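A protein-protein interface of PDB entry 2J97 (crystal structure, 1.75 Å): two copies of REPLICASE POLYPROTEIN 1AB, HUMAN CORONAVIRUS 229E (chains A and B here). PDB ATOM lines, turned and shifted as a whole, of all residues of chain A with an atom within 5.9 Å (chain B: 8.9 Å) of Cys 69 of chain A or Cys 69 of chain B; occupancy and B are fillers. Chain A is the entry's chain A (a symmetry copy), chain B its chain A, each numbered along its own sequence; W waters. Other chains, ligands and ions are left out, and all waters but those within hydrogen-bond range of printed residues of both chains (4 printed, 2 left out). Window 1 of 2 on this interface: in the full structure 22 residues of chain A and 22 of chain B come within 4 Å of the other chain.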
ATOM      1  N   PRO A  67     -27.375  23.016 -10.600  1.00  0.00           N
ATOM      2  CA  PRO A  67     -27.644  21.886 -11.507  1.00  0.00           C
ATOM      3  C   PRO A  67     -26.414  20.989 -11.603  1.00  0.00           C
ATOM      4  O   PRO A  67     -25.297  21.491 -11.619  1.00  0.00           O
ATOM      5  CB  PRO A  67     -27.934  22.570 -12.861  1.00  0.00           C
ATOM      6  CG  PRO A  67     -28.551  23.871 -12.476  1.00  0.00           C
ATOM      7  CD  PRO A  67     -27.767  24.302 -11.203  1.00  0.00           C
ATOM      8  N   PRO A  68     -26.629  19.663 -11.645  1.00  0.00           N
ATOM      9  CA  PRO A  68     -25.527  18.723 -11.422  1.00  0.00           C
ATOM     10  C   PRO A  68     -24.576  18.483 -12.582  1.00  0.00           C
ATOM     11  O   PRO A  68     -24.933  18.644 -13.743  1.00  0.00           O
ATOM     12  CB  PRO A  68     -26.244  17.413 -11.075  1.00  0.00           C
ATOM     13  CG  PRO A  68     -27.572  17.514 -11.763  1.00  0.00           C
ATOM     14  CD  PRO A  68     -27.926  18.977 -11.805  1.00  0.00           C
ATOM     15  N   CYS A  69     -23.390  18.044 -12.204  1.00  0.00           N
ATOM     16  CA  CYS A  69     -22.361  17.558 -13.084  1.00  0.00           C
ATOM     17  C   CYS A  69     -22.559  16.058 -13.128  1.00  0.00           C
ATOM     18  O   CYS A  69     -22.305  15.382 -12.112  1.00  0.00           O
ATOM     19  CB  CYS A  69     -21.013  17.876 -12.430  1.00  0.00           C
ATOM     20  SG  CYS A  69     -19.676  16.706 -12.825  1.00  0.00           S
ATOM     21  N   ARG A  70     -23.019  15.532 -14.260  1.00  0.00           N
ATOM     22  CA  ARG A  70     -23.114  14.084 -14.406  1.00  0.00           C
ATOM     23  C   ARG A  70     -21.746  13.522 -14.808  1.00  0.00           C
ATOM     24  O   ARG A  70     -21.052  14.095 -15.661  1.00  0.00           O
ATOM     25  CB  ARG A  70     -24.208  13.665 -15.415  1.00  0.00           C
ATOM     26  CG  ARG A  70     -23.941  13.963 -16.863  1.00  0.00           C
ATOM     27  CD  ARG A  70     -24.881  13.089 -17.754  1.00  0.00           C
ATOM     28  NE  ARG A  70     -24.247  11.839 -18.175  1.00  0.00           N
ATOM     29  CZ  ARG A  70     -24.851  10.894 -18.906  1.00  0.00           C
ATOM     30  NH1 ARG A  70     -26.126  11.033 -19.282  1.00  0.00           N
ATOM     31  NH2 ARG A  70     -24.183   9.817 -19.276  1.00  0.00           N
ATOM     32  N   PHE A  71     -21.339  12.414 -14.188  1.00  0.00           N
ATOM     33  CA  PHE A  71     -20.060  11.803 -14.558  1.00  0.00           C
ATOM     34  C   PHE A  71     -20.166  10.323 -14.324  1.00  0.00           C
ATOM     35  O   PHE A  71     -20.745   9.894 -13.340  1.00  0.00           O
ATOM     36  CB  PHE A  71     -18.855  12.384 -13.774  1.00  0.00           C
ATOM     37  CG  PHE A  71     -18.898  12.170 -12.278  1.00  0.00           C
ATOM     38  CD1 PHE A  71     -18.063  11.232 -11.664  1.00  0.00           C
ATOM     39  CD2 PHE A  71     -19.736  12.942 -11.457  1.00  0.00           C
ATOM     40  CE1 PHE A  71     -18.087  11.056 -10.296  1.00  0.00           C
ATOM     41  CE2 PHE A  71     -19.768  12.769 -10.067  1.00  0.00           C
ATOM     42  CZ  PHE A  71     -18.937  11.805  -9.479  1.00  0.00           C
ATOM     43  N   LYS A  82     -23.021   9.105 -11.879  1.00  0.00           N
ATOM     44  CA  LYS A  82     -23.129   9.834 -10.622  1.00  0.00           C
ATOM     45  C   LYS A  82     -23.462  11.288 -10.939  1.00  0.00           C
ATOM     46  O   LYS A  82     -23.201  11.757 -12.049  1.00  0.00           O
ATOM     47  CB  LYS A  82     -21.797   9.771  -9.860  1.00  0.00           C
ATOM     48  CG  LYS A  82     -21.257   8.348  -9.629  1.00  0.00           C
ATOM     49  CD  LYS A  82     -22.276   7.505  -8.884  1.00  0.00           C
ATOM     50  CE  LYS A  82     -21.829   6.046  -8.783  1.00  0.00           C
ATOM     51  NZ  LYS A  82     -22.895   5.231  -8.139  1.00  0.00           N
ATOM     52  N   TYR A  83     -24.029  11.987  -9.969  1.00  0.00           N
ATOM     53  CA  TYR A  83     -24.383  13.388 -10.133  1.00  0.00           C
ATOM     54  C   TYR A  83     -23.750  14.153  -8.993  1.00  0.00           C
ATOM     55  O   TYR A  83     -24.068  13.903  -7.838  1.00  0.00           O
ATOM     56  CB  TYR A  83     -25.897  13.536 -10.111  1.00  0.00           C
ATOM     57  CG  TYR A  83     -26.516  12.875 -11.315  1.00  0.00           C
ATOM     58  CD1 TYR A  83     -26.922  11.534 -11.287  1.00  0.00           C
ATOM     59  CD2 TYR A  83     -26.686  13.593 -12.495  1.00  0.00           C
ATOM     60  CE1 TYR A  83     -27.485  10.941 -12.415  1.00  0.00           C
ATOM     61  CE2 TYR A  83     -27.251  13.022 -13.617  1.00  0.00           C
ATOM     62  CZ  TYR A  83     -27.651  11.695 -13.574  1.00  0.00           C
ATOM     63  OH  TYR A  83     -28.188  11.166 -14.726  1.00  0.00           O
ATOM     64  N   LEU A  84     -22.880  15.102  -9.335  1.00  0.00           N
ATOM     65  CA  LEU A  84     -22.271  16.009  -8.364  1.00  0.00           C
ATOM     66  C   LEU A  84     -22.948  17.382  -8.362  1.00  0.00           C
ATOM     67  O   LEU A  84     -23.020  18.048  -9.410  1.00  0.00           O
ATOM     68  CB  LEU A  84     -20.785  16.189  -8.714  1.00  0.00           C
ATOM     69  CG  LEU A  84     -19.994  17.371  -8.143  1.00  0.00           C
ATOM     70  CD1 LEU A  84     -20.012  17.316  -6.615  1.00  0.00           C
ATOM     71  CD2 LEU A  84     -18.538  17.406  -8.714  1.00  0.00           C
ATOM     72  N   TYR A  85     -23.430  17.811  -7.199  1.00  0.00           N
ATOM     73  CA  TYR A  85     -24.108  19.099  -7.073  1.00  0.00           C
ATOM     74  C   TYR A  85     -23.294  19.996  -6.156  1.00  0.00           C
ATOM     75  O   TYR A  85     -23.079  19.643  -4.996  1.00  0.00           O
ATOM     76  CB  TYR A  85     -25.481  18.912  -6.411  1.00  0.00           C
ATOM     77  CG  TYR A  85     -26.503  18.072  -7.154  1.00  0.00           C
ATOM     78  CD1 TYR A  85     -26.448  16.670  -7.111  1.00  0.00           C
ATOM     79  CD2 TYR A  85     -27.566  18.675  -7.796  1.00  0.00           C
ATOM     80  CE1 TYR A  85     -27.424  15.893  -7.730  1.00  0.00           C
ATOM     81  CE2 TYR A  85     -28.560  17.908  -8.429  1.00  0.00           C
ATOM     82  CZ  TYR A  85     -28.475  16.520  -8.398  1.00  0.00           C
ATOM     83  OH  TYR A  85     -29.467  15.788  -9.032  1.00  0.00           O
ATOM     84  N   PHE A  86     -22.847  21.149  -6.641  1.00  0.00           N
ATOM     85  CA  PHE A  86     -22.175  22.081  -5.764  1.00  0.00           C
ATOM     86  C   PHE A  86     -23.248  22.890  -5.078  1.00  0.00           C
ATOM     87  O   PHE A  86     -24.312  23.125  -5.659  1.00  0.00           O
ATOM     88  CB  PHE A  86     -21.271  23.025  -6.579  1.00  0.00           C
ATOM     89  CG  PHE A  86     -20.046  22.374  -7.142  1.00  0.00           C
ATOM     90  CD1 PHE A  86     -19.931  22.180  -8.511  1.00  0.00           C
ATOM     91  CD2 PHE A  86     -19.002  21.984  -6.309  1.00  0.00           C
ATOM     92  CE1 PHE A  86     -18.766  21.592  -9.058  1.00  0.00           C
ATOM     93  CE2 PHE A  86     -17.844  21.404  -6.832  1.00  0.00           C
ATOM     94  CZ  PHE A  86     -17.712  21.212  -8.185  1.00  0.00           C
ATOM     95  N   LEU A  99     -13.675  18.744  -6.110  1.00  0.00           N
ATOM     96  CA  LEU A  99     -13.229  17.974  -7.275  1.00  0.00           C
ATOM     97  C   LEU A  99     -12.000  17.071  -6.963  1.00  0.00           C
ATOM     98  O   LEU A  99     -11.930  15.933  -7.428  1.00  0.00           O
ATOM     99  CB  LEU A  99     -12.893  18.900  -8.436  1.00  0.00           C
ATOM    100  CG  LEU A  99     -14.156  19.541  -9.057  1.00  0.00           C
ATOM    101  CD1 LEU A  99     -13.804  20.726  -9.968  1.00  0.00           C
ATOM    102  CD2 LEU A  99     -15.055  18.509  -9.785  1.00  0.00           C
ATOM    103  N   TYR B  42     -11.621  16.379 -22.011  1.00  0.00           N
ATOM    104  CA  TYR B  42     -11.746  17.601 -22.794  1.00  0.00           C
ATOM    105  C   TYR B  42     -12.606  18.566 -21.998  1.00  0.00           C
ATOM    106  O   TYR B  42     -13.668  18.175 -21.495  1.00  0.00           O
ATOM    107  CB  TYR B  42     -12.415  17.252 -24.116  1.00  0.00           C
ATOM    108  CG  TYR B  42     -12.613  18.397 -25.087  1.00  0.00           C
ATOM    109  CD1 TYR B  42     -11.516  19.137 -25.540  1.00  0.00           C
ATOM    110  CD2 TYR B  42     -13.885  18.717 -25.563  1.00  0.00           C
ATOM    111  CE1 TYR B  42     -11.662  20.170 -26.453  1.00  0.00           C
ATOM    112  CE2 TYR B  42     -14.065  19.799 -26.489  1.00  0.00           C
ATOM    113  CZ  TYR B  42     -12.916  20.502 -26.924  1.00  0.00           C
ATOM    114  OH  TYR B  42     -13.024  21.522 -27.840  1.00  0.00           O
ATOM    115  N   VAL B  43     -12.143  19.803 -21.853  1.00  0.00           N
ATOM    116  CA  VAL B  43     -12.933  20.843 -21.153  1.00  0.00           C
ATOM    117  C   VAL B  43     -13.222  21.967 -22.149  1.00  0.00           C
ATOM    118  O   VAL B  43     -12.297  22.545 -22.742  1.00  0.00           O
ATOM    119  CB  VAL B  43     -12.190  21.400 -19.930  1.00  0.00           C
ATOM    120  CG1 VAL B  43     -13.035  22.476 -19.189  1.00  0.00           C
ATOM    121  CG2 VAL B  43     -11.866  20.267 -18.937  1.00  0.00           C
ATOM    122  N   THR B  44     -14.494  22.309 -22.293  1.00  0.00           N
ATOM    123  CA  THR B  44     -14.875  23.406 -23.198  1.00  0.00           C
ATOM    124  C   THR B  44     -16.080  24.173 -22.629  1.00  0.00           C
ATOM    125  O   THR B  44     -16.411  24.028 -21.458  1.00  0.00           O
ATOM    126  CB  THR B  44     -15.060  22.887 -24.648  1.00  0.00           C
ATOM    127  OG1 THR B  44     -15.365  23.970 -25.526  1.00  0.00           O
ATOM    128  CG2 THR B  44     -16.196  21.829 -24.733  1.00  0.00           C
ATOM    129  N   LYS B  46     -19.225  24.589 -24.237  1.00  0.00           N
ATOM    130  CA  LYS B  46     -20.529  24.205 -24.778  1.00  0.00           C
ATOM    131  C   LYS B  46     -20.828  22.724 -24.589  1.00  0.00           C
ATOM    132  O   LYS B  46     -19.879  21.913 -24.552  1.00  0.00           O
ATOM    133  CB  LYS B  46     -20.702  24.627 -26.245  1.00  0.00           C
ATOM    134  CG  LYS B  46     -19.797  23.998 -27.248  1.00  0.00           C
ATOM    135  CD  LYS B  46     -20.304  24.257 -28.740  1.00  0.00           C
ATOM    136  CE  LYS B  46     -20.373  25.729 -29.163  1.00  0.00           C
ATOM    137  NZ  LYS B  46     -19.036  26.366 -29.396  1.00  0.00           N
ATOM    138  N   PRO B  47     -22.131  22.390 -24.467  1.00  0.00           N
ATOM    139  CA  PRO B  47     -22.628  21.023 -24.415  1.00  0.00           C
ATOM    140  C   PRO B  47     -22.692  20.454 -25.814  1.00  0.00           C
ATOM    141  O   PRO B  47     -22.466  21.162 -26.814  1.00  0.00           O
ATOM    142  CB  PRO B  47     -24.073  21.195 -23.887  1.00  0.00           C
ATOM    143  CG  PRO B  47     -24.490  22.539 -24.431  1.00  0.00           C
ATOM    144  CD  PRO B  47     -23.237  23.376 -24.406  1.00  0.00           C
ATOM    145  N   GLY B  48     -22.978  19.164 -25.876  1.00  0.00           N
ATOM    146  CA  GLY B  48     -23.320  18.534 -27.132  1.00  0.00           C
ATOM    147  C   GLY B  48     -22.154  18.018 -27.939  1.00  0.00           C
ATOM    148  O   GLY B  48     -22.366  17.490 -29.028  1.00  0.00           O
ATOM    149  N   GLU B  66     -17.707  10.994 -23.758  1.00  0.00           N
ATOM    150  CA  GLU B  66     -18.924  10.766 -22.959  1.00  0.00           C
ATOM    151  C   GLU B  66     -19.707  12.056 -22.790  1.00  0.00           C
ATOM    152  O   GLU B  66     -19.113  13.143 -22.831  1.00  0.00           O
ATOM    153  CB  GLU B  66     -18.556  10.220 -21.576  1.00  0.00           C
ATOM    154  CG  GLU B  66     -17.836   8.885 -21.666  1.00  0.00           C
ATOM    155  CD  GLU B  66     -17.444   8.335 -20.315  1.00  0.00           C
ATOM    156  OE1 GLU B  66     -17.453   9.099 -19.348  1.00  0.00           O
ATOM    157  OE2 GLU B  66     -17.129   7.129 -20.235  1.00  0.00           O
ATOM    158  N   PRO B  67     -21.035  11.958 -22.576  1.00  0.00           N
ATOM    159  CA  PRO B  67     -21.849  13.156 -22.305  1.00  0.00           C
ATOM    160  C   PRO B  67     -21.256  13.938 -21.138  1.00  0.00           C
ATOM    161  O   PRO B  67     -20.778  13.335 -20.185  1.00  0.00           O
ATOM    162  CB  PRO B  67     -23.233  12.579 -21.934  1.00  0.00           C
ATOM    163  CG  PRO B  67     -23.317  11.322 -22.731  1.00  0.00           C
ATOM    164  CD  PRO B  67     -21.871  10.749 -22.694  1.00  0.00           C
ATOM    165  N   PRO B  68     -21.271  15.279 -21.231  1.00  0.00           N
ATOM    166  CA  PRO B  68     -20.458  16.097 -20.328  1.00  0.00           C
ATOM    167  C   PRO B  68     -20.989  16.311 -18.921  1.00  0.00           C
ATOM    168  O   PRO B  68     -22.187  16.248 -18.674  1.00  0.00           O
ATOM    169  CB  PRO B  68     -20.378  17.448 -21.049  1.00  0.00           C
ATOM    170  CG  PRO B  68     -21.628  17.509 -21.876  1.00  0.00           C
ATOM    171  CD  PRO B  68     -21.973  16.090 -22.245  1.00  0.00           C
ATOM    172  N   CYS B  69     -20.046  16.615 -18.047  1.00  0.00           N
ATOM    173  CA  CYS B  69     -20.271  17.051 -16.695  1.00  0.00           C
ATOM    174  C   CYS B  69     -20.263  18.563 -16.763  1.00  0.00           C
ATOM    175  O   CYS B  69     -19.193  19.155 -17.000  1.00  0.00           O
ATOM    176  CB  CYS B  69     -19.082  16.572 -15.857  1.00  0.00           C
ATOM    177  SG  CYS B  69     -18.671  17.632 -14.436  1.00  0.00           S
ATOM    178  N   ARG B  70     -21.422  19.191 -16.583  1.00  0.00           N
ATOM    179  CA  ARG B  70     -21.460  20.647 -16.515  1.00  0.00           C
ATOM    180  C   ARG B  70     -21.098  21.099 -15.095  1.00  0.00           C
ATOM    181  O   ARG B  70     -21.560  20.512 -14.106  1.00  0.00           O
ATOM    182  CB  ARG B  70     -22.826  21.221 -16.951  1.00  0.00           C
ATOM    183  CG  ARG B  70     -23.987  20.980 -16.030  1.00  0.00           C
ATOM    184  CD  ARG B  70     -25.135  21.986 -16.365  1.00  0.00           C
ATOM    185  NE  ARG B  70     -25.078  23.194 -15.539  1.00  0.00           N
ATOM    186  CZ  ARG B  70     -25.919  24.229 -15.656  1.00  0.00           C
ATOM    187  NH1 ARG B  70     -26.874  24.231 -16.590  1.00  0.00           N
ATOM    188  NH2 ARG B  70     -25.817  25.258 -14.834  1.00  0.00           N
ATOM    189  N   PHE B  71     -20.258  22.129 -14.982  1.00  0.00           N
ATOM    190  CA  PHE B  71     -19.906  22.636 -13.654  1.00  0.00           C
ATOM    191  C   PHE B  71     -19.615  24.105 -13.779  1.00  0.00           C
ATOM    192  O   PHE B  71     -18.997  24.532 -14.741  1.00  0.00           O
ATOM    193  CB  PHE B  71     -18.698  21.902 -13.019  1.00  0.00           C
ATOM    194  CG  PHE B  71     -17.395  22.038 -13.775  1.00  0.00           C
ATOM    195  CD1 PHE B  71     -16.369  22.858 -13.295  1.00  0.00           C
ATOM    196  CD2 PHE B  71     -17.156  21.303 -14.948  1.00  0.00           C
ATOM    197  CE1 PHE B  71     -15.173  22.960 -13.974  1.00  0.00           C
ATOM    198  CE2 PHE B  71     -15.944  21.402 -15.645  1.00  0.00           C
ATOM    199  CZ  PHE B  71     -14.941  22.249 -15.154  1.00  0.00           C
ATOM    200  N   VAL B  72     -20.092  24.852 -12.791  1.00  0.00           N
ATOM    201  CA  VAL B  72     -19.844  26.288 -12.677  1.00  0.00           C
ATOM    202  C   VAL B  72     -18.510  26.582 -12.011  1.00  0.00           C
ATOM    203  O   VAL B  72     -18.095  25.903 -11.069  1.00  0.00           O
ATOM    204  CB  VAL B  72     -20.978  26.946 -11.906  1.00  0.00           C
ATOM    205  CG1 VAL B  72     -20.608  28.355 -11.384  1.00  0.00           C
ATOM    206  CG2 VAL B  72     -22.228  27.010 -12.818  1.00  0.00           C
ATOM    207  N   ILE B  81     -20.320  28.519 -16.921  1.00  0.00           N
ATOM    208  CA  ILE B  81     -20.496  27.064 -17.002  1.00  0.00           C
ATOM    209  C   ILE B  81     -19.448  26.452 -17.927  1.00  0.00           C
ATOM    210  O   ILE B  81     -19.276  26.899 -19.078  1.00  0.00           O
ATOM    211  CB  ILE B  81     -21.908  26.687 -17.583  1.00  0.00           C
ATOM    212  CG1 ILE B  81     -23.009  27.340 -16.741  1.00  0.00           C
ATOM    213  CG2 ILE B  81     -22.062  25.149 -17.647  1.00  0.00           C
ATOM    214  CD1 ILE B  81     -24.401  27.236 -17.396  1.00  0.00           C
ATOM    215  N   LYS B  82     -18.747  25.448 -17.393  1.00  0.00           N
ATOM    216  CA  LYS B  82     -17.772  24.665 -18.140  1.00  0.00           C
ATOM    217  C   LYS B  82     -18.345  23.268 -18.354  1.00  0.00           C
ATOM    218  O   LYS B  82     -19.231  22.839 -17.612  1.00  0.00           O
ATOM    219  CB  LYS B  82     -16.461  24.561 -17.348  1.00  0.00           C
ATOM    220  CG  LYS B  82     -15.866  25.912 -16.911  1.00  0.00           C
ATOM    221  CD  LYS B  82     -15.629  26.804 -18.116  1.00  0.00           C
ATOM    222  CE  LYS B  82     -15.189  28.207 -17.696  1.00  0.00           C
ATOM    223  NZ  LYS B  82     -15.065  29.082 -18.894  1.00  0.00           N
ATOM    224  N   TYR B  83     -17.838  22.573 -19.360  1.00  0.00           N
ATOM    225  CA  TYR B  83     -18.285  21.222 -19.666  1.00  0.00           C
ATOM    226  C   TYR B  83     -17.057  20.340 -19.714  1.00  0.00           C
ATOM    227  O   TYR B  83     -16.181  20.554 -20.540  1.00  0.00           O
ATOM    228  CB  TYR B  83     -19.009  21.216 -21.004  1.00  0.00           C
ATOM    229  CG  TYR B  83     -20.293  21.998 -20.919  1.00  0.00           C
ATOM    230  CD1 TYR B  83     -20.338  23.367 -21.213  1.00  0.00           C
ATOM    231  CD2 TYR B  83     -21.470  21.365 -20.531  1.00  0.00           C
ATOM    232  CE1 TYR B  83     -21.537  24.072 -21.120  1.00  0.00           C
ATOM    233  CE2 TYR B  83     -22.667  22.048 -20.445  1.00  0.00           C
ATOM    234  CZ  TYR B  83     -22.698  23.402 -20.741  1.00  0.00           C
ATOM    235  OH  TYR B  83     -23.911  24.041 -20.617  1.00  0.00           O
ATOM    236  N   LEU B  84     -17.024  19.334 -18.841  1.00  0.00           N
ATOM    237  CA  LEU B  84     -15.970  18.322 -18.834  1.00  0.00           C
ATOM    238  C   LEU B  84     -16.423  17.020 -19.501  1.00  0.00           C
ATOM    239  O   LEU B  84     -17.433  16.423 -19.088  1.00  0.00           O
ATOM    240  CB  LEU B  84     -15.576  18.022 -17.379  1.00  0.00           C
ATOM    241  CG  LEU B  84     -14.808  16.742 -17.034  1.00  0.00           C
ATOM    242  CD1 LEU B  84     -13.480  16.715 -17.792  1.00  0.00           C
ATOM    243  CD2 LEU B  84     -14.606  16.602 -15.489  1.00  0.00           C
ATOM    244  N   TYR B  85     -15.683  16.575 -20.511  1.00  0.00           N
ATOM    245  CA  TYR B  85     -16.021  15.352 -21.235  1.00  0.00           C
ATOM    246  C   TYR B  85     -14.914  14.333 -21.022  1.00  0.00           C
ATOM    247  O   TYR B  85     -13.767  14.599 -21.381  1.00  0.00           O
ATOM    248  CB  TYR B  85     -16.089  15.629 -22.743  1.00  0.00           C
ATOM    249  CG  TYR B  85     -17.151  16.601 -23.225  1.00  0.00           C
ATOM    250  CD1 TYR B  85     -16.955  17.988 -23.121  1.00  0.00           C
ATOM    251  CD2 TYR B  85     -18.278  16.137 -23.871  1.00  0.00           C
ATOM    252  CE1 TYR B  85     -17.891  18.885 -23.626  1.00  0.00           C
ATOM    253  CE2 TYR B  85     -19.237  17.027 -24.385  1.00  0.00           C
ATOM    254  CZ  TYR B  85     -19.039  18.398 -24.250  1.00  0.00           C
ATOM    255  OH  TYR B  85     -20.000  19.253 -24.764  1.00  0.00           O
ATOM    256  N   PHE B  86     -15.229  13.171 -20.460  1.00  0.00           N
ATOM    257  CA  PHE B  86     -14.228  12.133 -20.354  1.00  0.00           C
ATOM    258  C   PHE B  86     -14.224  11.392 -21.667  1.00  0.00           C
ATOM    259  O   PHE B  86     -15.265  11.290 -22.324  1.00  0.00           O
ATOM    260  CB  PHE B  86     -14.591  11.156 -19.221  1.00  0.00           C
ATOM    261  CG  PHE B  86     -14.430  11.718 -17.843  1.00  0.00           C
ATOM    262  CD1 PHE B  86     -15.549  11.976 -17.064  1.00  0.00           C
ATOM    263  CD2 PHE B  86     -13.164  11.963 -17.319  1.00  0.00           C
ATOM    264  CE1 PHE B  86     -15.409  12.482 -15.750  1.00  0.00           C
ATOM    265  CE2 PHE B  86     -13.008  12.459 -16.022  1.00  0.00           C
ATOM    266  CZ  PHE B  86     -14.105  12.713 -15.237  1.00  0.00           C
ATOM    267  N   VAL B  98      -7.934  13.219 -13.706  1.00  0.00           N
ATOM    268  CA  VAL B  98      -8.528  14.372 -14.408  1.00  0.00           C
ATOM    269  C   VAL B  98      -9.263  15.261 -13.423  1.00  0.00           C
ATOM    270  O   VAL B  98      -9.076  16.479 -13.425  1.00  0.00           O
ATOM    271  CB  VAL B  98      -9.483  13.918 -15.535  1.00  0.00           C
ATOM    272  CG1 VAL B  98     -10.327  15.093 -16.032  1.00  0.00           C
ATOM    273  CG2 VAL B  98      -8.662  13.306 -16.707  1.00  0.00           C
ATOM    274  N   LEU B  99     -10.120  14.673 -12.597  1.00  0.00           N
ATOM    275  CA  LEU B  99     -10.847  15.462 -11.597  1.00  0.00           C
ATOM    276  C   LEU B  99      -9.899  16.226 -10.629  1.00  0.00           C
ATOM    277  O   LEU B  99     -10.164  17.376 -10.279  1.00  0.00           O
ATOM    278  CB  LEU B  99     -11.783  14.573 -10.789  1.00  0.00           C
ATOM    279  CG  LEU B  99     -12.993  14.089 -11.622  1.00  0.00           C
ATOM    280  CD1 LEU B  99     -13.728  12.928 -10.936  1.00  0.00           C
ATOM    281  CD2 LEU B  99     -13.965  15.238 -11.993  1.00  0.00           C
ATOM    282  N   ILE B 102      -8.299  19.191 -12.544  1.00  0.00           N
ATOM    283  CA  ILE B 102      -9.256  20.287 -12.671  1.00  0.00           C
ATOM    284  C   ILE B 102      -9.480  20.964 -11.327  1.00  0.00           C
ATOM    285  O   ILE B 102      -9.513  22.184 -11.243  1.00  0.00           O
ATOM    286  CB  ILE B 102     -10.574  19.807 -13.294  1.00  0.00           C
ATOM    287  CG1 ILE B 102     -10.300  19.337 -14.726  1.00  0.00           C
ATOM    288  CG2 ILE B 102     -11.668  20.902 -13.219  1.00  0.00           C
ATOM    289  CD1 ILE B 102     -11.465  18.678 -15.411  1.00  0.00           C
HETATM  290  O   HOH W   1     -24.418  23.923 -12.550  1.00  0.00           O
HETATM  291  O   HOH W   2     -21.394  10.887 -19.097  1.00  0.00           O
HETATM  292  O   HOH W   3     -22.489  21.290 -11.719  1.00  0.00           O
HETATM  293  O   HOH W   4     -19.494  13.278 -17.678  1.00  0.00           O
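The backbone NH (N) of Glu 66 of chain B sits at hydrogen-bond distance from the backbone carbonyl oxygen (O) of Phe 86 of chain B. The backbone carbonyl oxygen (O) of Leu 84 of chain B lies within hydrogen-bond range of the backbone NH (N) of Cys 69 of chain B, 2.8 Å away. O of Phe 71 of chain B is in hydrogen-bond range of N of Lys 82 of chain B (2.8 Å). N of Cys 69 of chain A lies within hydrogen-bond range of O of Leu 84 of chain A, 2.8 Å away. N of Lys 82 of chain A sits at hydrogen-bond distance from O of Phe 71 of chain A, at 2.8 Å.
SG of Cys 69 of chain B is disulfide-bonded to SG of Cys 69 of chain A (2.1 Å).
Among the printed residues, merely in contact across the chains: Pro 67 of chain A with Arg 70 of chain B (3.8 Å), Pro 68 of chain A with Arg 70 of chain B (3.4 Å), Cys 69 of chain A with Arg 70 of chain B (3.2 Å), Arg 70 of chain A with Pro 67 of chain B (3.8 Å), Arg 70 of chain A with Pro 68 of chain B (3.4 Å), Arg 70 of chain A with Cys 69 of chain B (3.2 Å), Phe 71 of chain A with Phe 86 of chain B (3.97 Å), Phe 86 of chain A with Phe 71 of chain B (3.97 Å), Leu 99 of chain A with Leu 99 of chain B (3.6 Å) and Leu 99 of chain A with Ile 102 of chain B (3.9 Å).
Printed residues of chain A that touch a printed residue of chain B: Pro 67, Pro 68, Cys 69, Arg 70, Phe 71, Phe 86 and Leu 99. Hydrophobic or aromatic side chains of chain A within 4 Å of the printed part of chain B: Pro 67, Phe 71, Phe 86 and Leu 99. Hydrophobic or aromatic side chains of chain B that line the printed part of chain A: Pro 67, Phe 71, Phe 86, Leu 99 and Ile 102.
Pro 67 of chain A touches Arg 70 of chain B, and with the chains exchanged Arg 70 of chain A touches Pro 67 of chain B. Pro 68 of chain A touches Arg 70 of chain B, and with the chains exchanged Arg 70 of chain A touches Pro 68 of chain B. Cys 69 of chain A touches Arg 70 of chain B, and with the chains exchanged Arg 70 of chain A touches Cys 69 of chain B. Leu 99 of chain B touches its own counterpart, Leu 99 of chain A. Positions printed for both chains: 67, 68, 69, 70, 71, 82, 83, 84, 85, 86 and 99.
Cys 69 of chain A touches just these residues of chain B: Cys 69 (2.1 Å) and Arg 70 (3.2 Å). Of the printed residues of chain A, Cys 69 of chain B touches Cys 69 and Arg 70. Pro 68 of chain A touches one residue of chain B. Printed residues of chain B within 4 Å of Phe 86 of chain A: Phe 71 (3.97 Å). Printed residues of chain B within 4 Å of Leu 99 of chain A: Leu 99 (3.6 Å) and Ile 102 (3.9 Å). The nearest residue of chain A that does not touch Cys 69 of chain B is Phe 71 of chain A (4.7 Å).
Water W4 lies within hydrogen-bond range of the backbone carbonyl oxygen (O) of Arg 70 of chain A (2.7 Å), the backbone carbonyl oxygen (O) of Pro 67 of chain B (2.8 Å) and the backbone NH (N) of Cys 69 of chain B (3.4 Å). Water W3 lies within hydrogen-bond range of O of Arg 70 of chain B, O of Pro 67 of chain A and N of Cys 69 of chain A. Water W1 lies within hydrogen-bond range of O of Pro 67 of chain A (2.7 Å) and NH2 of Arg 70 of chain B (3.0 Å). Water W2 bridges the backbone carbonyl oxygen of Pro 67 of chain B (2.7 Å) and the guanidinium group of Arg 70 of chain A (3.0 Å).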
